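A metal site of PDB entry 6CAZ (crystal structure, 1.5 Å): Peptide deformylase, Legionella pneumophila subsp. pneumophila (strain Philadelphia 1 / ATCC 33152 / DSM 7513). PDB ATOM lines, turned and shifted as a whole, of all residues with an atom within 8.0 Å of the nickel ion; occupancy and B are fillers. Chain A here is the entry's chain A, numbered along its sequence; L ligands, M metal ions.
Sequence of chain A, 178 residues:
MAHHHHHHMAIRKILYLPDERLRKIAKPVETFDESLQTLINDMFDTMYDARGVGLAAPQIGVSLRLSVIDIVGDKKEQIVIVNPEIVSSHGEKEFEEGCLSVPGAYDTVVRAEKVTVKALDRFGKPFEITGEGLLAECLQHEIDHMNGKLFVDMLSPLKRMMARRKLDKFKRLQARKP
Residues that only touch the nickel ion: Gln 59. The nearest printed residue that does not touch the nickel ion is Leu 100 (4.004 Å).
ND1 of His 141 sits at hydrogen-bond distance from OE2 of Glu 97, at 2.7 Å. A ring nitrogen (NE2) of His 145 sits close to the side-chain amide nitrogen (NE2) of Gln 59, 3.4 Å away. SG of Cys 99 lies close to N of Ser 101, 3.4 Å away. The side-chain hydroxyl (OG) of Ser 101 sits at hydrogen-bond distance from the side-chain amide nitrogen (NE2) of Gln 59 (3.1 Å). The backbone NH (N) of Ala 56 sits at hydrogen-bond distance from the side-chain amide oxygen (OE1) of Gln 59 (2.9 Å). The backbone carbonyl oxygen (O) of Gln 59 is in hydrogen-bond range of the backbone NH (N) of Leu 15.
NE2 of His 141 binds the nickel ion. A ring nitrogen (NE2) of His 145 is bound to the nickel ion, at 2.1 Å. The nickel ion is bound by SG of Cys 99 (2.3 Å). CL1 of the ligand binds the nickel ion (2.3 Å).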
ATOM      1  N   ILE A  14      14.995   9.544  -1.640  1.00  0.00           N
ATOM      2  CA  ILE A  14      14.791   9.653  -3.075  1.00  0.00           C
ATOM      3  C   ILE A  14      15.428   8.445  -3.745  1.00  0.00           C
ATOM      4  O   ILE A  14      16.564   8.055  -3.414  1.00  0.00           O
ATOM      5  CB  ILE A  14      15.384  10.960  -3.602  1.00  0.00           C
ATOM      6  CG1 ILE A  14      14.641  12.142  -2.977  1.00  0.00           C
ATOM      7  CG2 ILE A  14      15.296  11.039  -5.130  1.00  0.00           C
ATOM      8  CD1 ILE A  14      15.162  13.492  -3.354  1.00  0.00           C
ATOM      9  N   LEU A  15      14.699   7.814  -4.652  1.00  0.00           N
ATOM     10  CA  LEU A  15      15.204   6.672  -5.401  1.00  0.00           C
ATOM     11  C   LEU A  15      16.064   7.130  -6.569  1.00  0.00           C
ATOM     12  O   LEU A  15      15.818   8.175  -7.188  1.00  0.00           O
ATOM     13  CB  LEU A  15      14.038   5.868  -5.956  1.00  0.00           C
ATOM     14  CG  LEU A  15      12.997   5.355  -4.957  1.00  0.00           C
ATOM     15  CD1 LEU A  15      12.078   4.357  -5.631  1.00  0.00           C
ATOM     16  CD2 LEU A  15      13.659   4.743  -3.743  1.00  0.00           C
ATOM     17  N   LEU A  22      11.164   3.572 -10.521  1.00  0.00           N
ATOM     18  CA  LEU A  22      11.154   4.777 -11.335  1.00  0.00           C
ATOM     19  C   LEU A  22      10.656   4.524 -12.743  1.00  0.00           C
ATOM     20  O   LEU A  22      10.385   5.494 -13.466  1.00  0.00           O
ATOM     21  CB  LEU A  22      12.579   5.360 -11.396  1.00  0.00           C
ATOM     22  CG  LEU A  22      13.173   5.849 -10.067  1.00  0.00           C
ATOM     23  CD1 LEU A  22      14.687   6.084 -10.198  1.00  0.00           C
ATOM     24  CD2 LEU A  22      12.464   7.114  -9.585  1.00  0.00           C
ATOM     25  N   GLY A  54      10.808  20.426  -7.875  1.00  0.00           N
ATOM     26  CA  GLY A  54       9.721  19.505  -8.138  1.00  0.00           C
ATOM     27  C   GLY A  54      10.093  18.113  -7.674  1.00  0.00           C
ATOM     28  O   GLY A  54      11.275  17.740  -7.617  1.00  0.00           O
ATOM     29  N   LEU A  55       9.079  17.326  -7.350  1.00  0.00           N
ATOM     30  CA  LEU A  55       9.288  15.941  -6.953  1.00  0.00           C
ATOM     31  C   LEU A  55       8.020  15.177  -7.301  1.00  0.00           C
ATOM     32  O   LEU A  55       6.923  15.641  -7.017  1.00  0.00           O
ATOM     33  CB  LEU A  55       9.575  15.834  -5.451  1.00  0.00           C
ATOM     34  CG  LEU A  55       9.942  14.431  -4.952  1.00  0.00           C
ATOM     35  CD1 LEU A  55      11.338  14.036  -5.430  1.00  0.00           C
ATOM     36  CD2 LEU A  55       9.874  14.376  -3.430  1.00  0.00           C
ATOM     37  N   ALA A  56       8.190  14.000  -7.909  1.00  0.00           N
ATOM     38  CA  ALA A  56       7.065  13.136  -8.256  1.00  0.00           C
ATOM     39  C   ALA A  56       7.019  11.934  -7.317  1.00  0.00           C
ATOM     40  O   ALA A  56       8.058  11.430  -6.869  1.00  0.00           O
ATOM     41  CB  ALA A  56       7.184  12.643  -9.709  1.00  0.00           C
ATOM     42  N   GLN A  59       9.389   8.988  -7.364  1.00  0.00           N
ATOM     43  CA  GLN A  59      10.754   9.211  -6.912  1.00  0.00           C
ATOM     44  C   GLN A  59      10.976   8.912  -5.432  1.00  0.00           C
ATOM     45  O   GLN A  59      12.131   8.857  -5.008  1.00  0.00           O
ATOM     46  CB  GLN A  59      11.160  10.655  -7.180  1.00  0.00           C
ATOM     47  CG  GLN A  59      11.269  10.988  -8.648  1.00  0.00           C
ATOM     48  CD  GLN A  59      11.661  12.423  -8.832  1.00  0.00           C
ATOM     49  OE1 GLN A  59      10.799  13.316  -8.936  1.00  0.00           O
ATOM     50  NE2 GLN A  59      12.954  12.667  -8.855  1.00  0.00           N
ATOM     51  N   GLU A  97      19.390  20.233 -18.121  1.00  0.00           N
ATOM     52  CA  GLU A  97      18.504  19.604 -17.163  1.00  0.00           C
ATOM     53  C   GLU A  97      19.253  18.624 -16.255  1.00  0.00           C
ATOM     54  O   GLU A  97      20.233  18.001 -16.648  1.00  0.00           O
ATOM     55  CB  GLU A  97      17.403  18.856 -17.911  1.00  0.00           C
ATOM     56  CG  GLU A  97      16.301  18.325 -17.011  1.00  0.00           C
ATOM     57  CD  GLU A  97      15.018  17.998 -17.757  1.00  0.00           C
ATOM     58  OE1 GLU A  97      14.439  18.889 -18.414  1.00  0.00           O
ATOM     59  OE2 GLU A  97      14.603  16.829 -17.685  1.00  0.00           O
ATOM     60  N   GLY A  98      18.758  18.507 -15.015  1.00  0.00           N
ATOM     61  CA  GLY A  98      19.151  17.440 -14.112  1.00  0.00           C
ATOM     62  C   GLY A  98      17.918  16.752 -13.546  1.00  0.00           C
ATOM     63  O   GLY A  98      16.784  17.061 -13.907  1.00  0.00           O
ATOM     64  N   CYS A  99      18.179  15.825 -12.626  1.00  0.00           N
ATOM     65  CA  CYS A  99      17.094  15.067 -12.004  1.00  0.00           C
ATOM     66  C   CYS A  99      17.567  14.557 -10.657  1.00  0.00           C
ATOM     67  O   CYS A  99      18.662  13.979 -10.569  1.00  0.00           O
ATOM     68  CB  CYS A  99      16.737  13.853 -12.878  1.00  0.00           C
ATOM     69  SG  CYS A  99      15.379  12.802 -12.222  1.00  0.00           S
ATOM     70  N   LEU A 100      16.723  14.720  -9.626  1.00  0.00           N
ATOM     71  CA  LEU A 100      17.054  14.235  -8.288  1.00  0.00           C
ATOM     72  C   LEU A 100      17.243  12.722  -8.245  1.00  0.00           C
ATOM     73  O   LEU A 100      17.924  12.218  -7.339  1.00  0.00           O
ATOM     74  CB  LEU A 100      15.967  14.645  -7.291  1.00  0.00           C
ATOM     75  CG  LEU A 100      15.795  16.145  -7.102  1.00  0.00           C
ATOM     76  CD1 LEU A 100      14.604  16.420  -6.209  1.00  0.00           C
ATOM     77  CD2 LEU A 100      17.060  16.733  -6.501  1.00  0.00           C
ATOM     78  N   SER A 101      16.654  11.992  -9.188  1.00  0.00           N
ATOM     79  CA  SER A 101      16.809  10.548  -9.263  1.00  0.00           C
ATOM     80  C   SER A 101      17.943  10.115 -10.167  1.00  0.00           C
ATOM     81  O   SER A 101      18.179   8.917 -10.325  1.00  0.00           O
ATOM     82  CB  SER A 101      15.490   9.905  -9.711  1.00  0.00           C
ATOM     83  OG  SER A 101      14.505  10.023  -8.690  1.00  0.00           O
ATOM     84  N   VAL A 102      18.649  11.064 -10.788  1.00  0.00           N
ATOM     85  CA  VAL A 102      19.895  10.777 -11.496  1.00  0.00           C
ATOM     86  C   VAL A 102      20.949  11.764 -10.983  1.00  0.00           C
ATOM     87  O   VAL A 102      21.474  12.569 -11.760  1.00  0.00           O
ATOM     88  CB  VAL A 102      19.731  10.871 -13.030  1.00  0.00           C
ATOM     89  CG1 VAL A 102      20.915  10.178 -13.720  1.00  0.00           C
ATOM     90  CG2 VAL A 102      18.426  10.228 -13.481  1.00  0.00           C
ATOM     91  N   ARG A 111      12.325  19.899 -24.945  1.00  0.00           N
ATOM     92  CA  ARG A 111      10.941  19.797 -24.489  1.00  0.00           C
ATOM     93  C   ARG A 111      10.142  20.952 -25.084  1.00  0.00           C
ATOM     94  O   ARG A 111      10.681  21.843 -25.737  1.00  0.00           O
ATOM     95  CB  ARG A 111      10.834  19.828 -22.969  1.00  0.00           C
ATOM     96  CG  ARG A 111      11.673  18.765 -22.236  1.00  0.00           C
ATOM     97  CD  ARG A 111      11.402  18.854 -20.745  1.00  0.00           C
ATOM     98  NE  ARG A 111      12.139  17.869 -19.944  1.00  0.00           N
ATOM     99  CZ  ARG A 111      11.765  16.602 -19.810  1.00  0.00           C
ATOM    100  NH1 ARG A 111      10.685  16.147 -20.436  1.00  0.00           N
ATOM    101  NH2 ARG A 111      12.474  15.783 -19.034  1.00  0.00           N
ATOM    102  N   CYS A 138       9.669  21.853 -15.733  1.00  0.00           N
ATOM    103  CA  CYS A 138       9.378  21.032 -14.561  1.00  0.00           C
ATOM    104  C   CYS A 138       8.101  20.226 -14.750  1.00  0.00           C
ATOM    105  O   CYS A 138       8.067  19.031 -14.447  1.00  0.00           O
ATOM    106  CB  CYS A 138       9.291  21.922 -13.325  1.00  0.00           C
ATOM    107  SG  CYS A 138       9.029  21.011 -11.795  1.00  0.00           S
ATOM    108  N   HIS A 141       8.819  17.359 -17.040  1.00  0.00           N
ATOM    109  CA  HIS A 141       9.700  16.431 -16.351  1.00  0.00           C
ATOM    110  C   HIS A 141       8.935  15.609 -15.319  1.00  0.00           C
ATOM    111  O   HIS A 141       9.143  14.395 -15.183  1.00  0.00           O
ATOM    112  CB  HIS A 141      10.797  17.267 -15.690  1.00  0.00           C
ATOM    113  CG  HIS A 141      11.841  16.477 -14.975  1.00  0.00           C
ATOM    114  ND1 HIS A 141      13.087  16.223 -15.506  1.00  0.00           N
ATOM    115  CD2 HIS A 141      11.827  15.919 -13.742  1.00  0.00           C
ATOM    116  CE1 HIS A 141      13.796  15.513 -14.633  1.00  0.00           C
ATOM    117  NE2 HIS A 141      13.049  15.309 -13.561  1.00  0.00           N
ATOM    118  N   GLU A 142       7.990  16.240 -14.615  1.00  0.00           N
ATOM    119  CA  GLU A 142       7.169  15.561 -13.610  1.00  0.00           C
ATOM    120  C   GLU A 142       6.265  14.523 -14.258  1.00  0.00           C
ATOM    121  O   GLU A 142       6.150  13.387 -13.778  1.00  0.00           O
ATOM    122  CB  GLU A 142       6.296  16.564 -12.863  1.00  0.00           C
ATOM    123  CG  GLU A 142       7.041  17.547 -11.989  1.00  0.00           C
ATOM    124  CD  GLU A 142       8.034  16.864 -11.087  1.00  0.00           C
ATOM    125  OE1 GLU A 142       7.664  15.839 -10.477  1.00  0.00           O
ATOM    126  OE2 GLU A 142       9.177  17.344 -11.008  1.00  0.00           O
ATOM    127  N   ASP A 144       6.676  13.056 -17.096  1.00  0.00           N
ATOM    128  CA  ASP A 144       7.559  11.963 -17.504  1.00  0.00           C
ATOM    129  C   ASP A 144       7.800  10.986 -16.356  1.00  0.00           C
ATOM    130  O   ASP A 144       7.730   9.767 -16.541  1.00  0.00           O
ATOM    131  CB  ASP A 144       8.895  12.491 -18.031  1.00  0.00           C
ATOM    132  CG  ASP A 144       8.824  12.992 -19.465  1.00  0.00           C
ATOM    133  OD1 ASP A 144       7.742  12.982 -20.097  1.00  0.00           O
ATOM    134  OD2 ASP A 144       9.887  13.424 -19.960  1.00  0.00           O
ATOM    135  N   HIS A 145       8.100  11.507 -15.145  1.00  0.00           N
ATOM    136  CA  HIS A 145       8.337  10.611 -14.004  1.00  0.00           C
ATOM    137  C   HIS A 145       7.131   9.715 -13.757  1.00  0.00           C
ATOM    138  O   HIS A 145       7.282   8.554 -13.357  1.00  0.00           O
ATOM    139  CB  HIS A 145       8.596  11.419 -12.740  1.00  0.00           C
ATOM    140  CG  HIS A 145      10.031  11.768 -12.509  1.00  0.00           C
ATOM    141  ND1 HIS A 145      11.043  10.841 -12.451  1.00  0.00           N
ATOM    142  CD2 HIS A 145      10.611  12.974 -12.307  1.00  0.00           C
ATOM    143  CE1 HIS A 145      12.198  11.453 -12.219  1.00  0.00           C
ATOM    144  NE2 HIS A 145      11.955  12.755 -12.135  1.00  0.00           N
ATOM    145  N   LYS A 149       9.553   7.605 -17.274  1.00  0.00           N
ATOM    146  CA  LYS A 149      10.530   8.161 -18.201  1.00  0.00           C
ATOM    147  C   LYS A 149      11.454   9.094 -17.432  1.00  0.00           C
ATOM    148  O   LYS A 149      10.997   9.913 -16.625  1.00  0.00           O
ATOM    149  CB  LYS A 149       9.836   8.926 -19.319  1.00  0.00           C
ATOM    150  CG  LYS A 149      10.786   9.678 -20.242  1.00  0.00           C
ATOM    151  CD  LYS A 149      10.042  10.201 -21.474  1.00  0.00           C
ATOM    152  CE  LYS A 149      10.992  10.907 -22.428  1.00  0.00           C
ATOM    153  NZ  LYS A 149      10.247  11.584 -23.532  1.00  0.00           N
ATOM    154  N   LEU A 150      12.754   8.954 -17.682  1.00  0.00           N
ATOM    155  CA  LEU A 150      13.785   9.770 -17.054  1.00  0.00           C
ATOM    156  C   LEU A 150      14.517  10.512 -18.171  1.00  0.00           C
ATOM    157  O   LEU A 150      14.573  10.036 -19.296  1.00  0.00           O
ATOM    158  CB  LEU A 150      14.779   8.892 -16.289  1.00  0.00           C
ATOM    159  CG  LEU A 150      14.161   8.016 -15.202  1.00  0.00           C
ATOM    160  CD1 LEU A 150      15.170   6.984 -14.655  1.00  0.00           C
ATOM    161  CD2 LEU A 150      13.701   8.941 -14.107  1.00  0.00           C
ATOM    162  N   PHE A 151      15.078  11.687 -17.843  1.00  0.00           N
ATOM    163  CA  PHE A 151      15.561  12.553 -18.916  1.00  0.00           C
ATOM    164  C   PHE A 151      16.717  11.935 -19.679  1.00  0.00           C
ATOM    165  O   PHE A 151      16.921  12.227 -20.864  1.00  0.00           O
ATOM    166  CB  PHE A 151      15.904  13.956 -18.388  1.00  0.00           C
ATOM    167  CG  PHE A 151      17.271  14.067 -17.769  1.00  0.00           C
ATOM    168  CD1 PHE A 151      17.503  13.660 -16.464  1.00  0.00           C
ATOM    169  CD2 PHE A 151      18.337  14.595 -18.496  1.00  0.00           C
ATOM    170  CE1 PHE A 151      18.778  13.763 -15.894  1.00  0.00           C
ATOM    171  CE2 PHE A 151      19.610  14.710 -17.933  1.00  0.00           C
ATOM    172  CZ  PHE A 151      19.829  14.285 -16.625  1.00  0.00           C
HETATM  173 CL1  LIG L   1      13.682  15.549 -10.207  1.00  0.00          CL
HETATM  174 NI    NI M   1      13.540  14.121 -11.980  1.00  0.00          NI
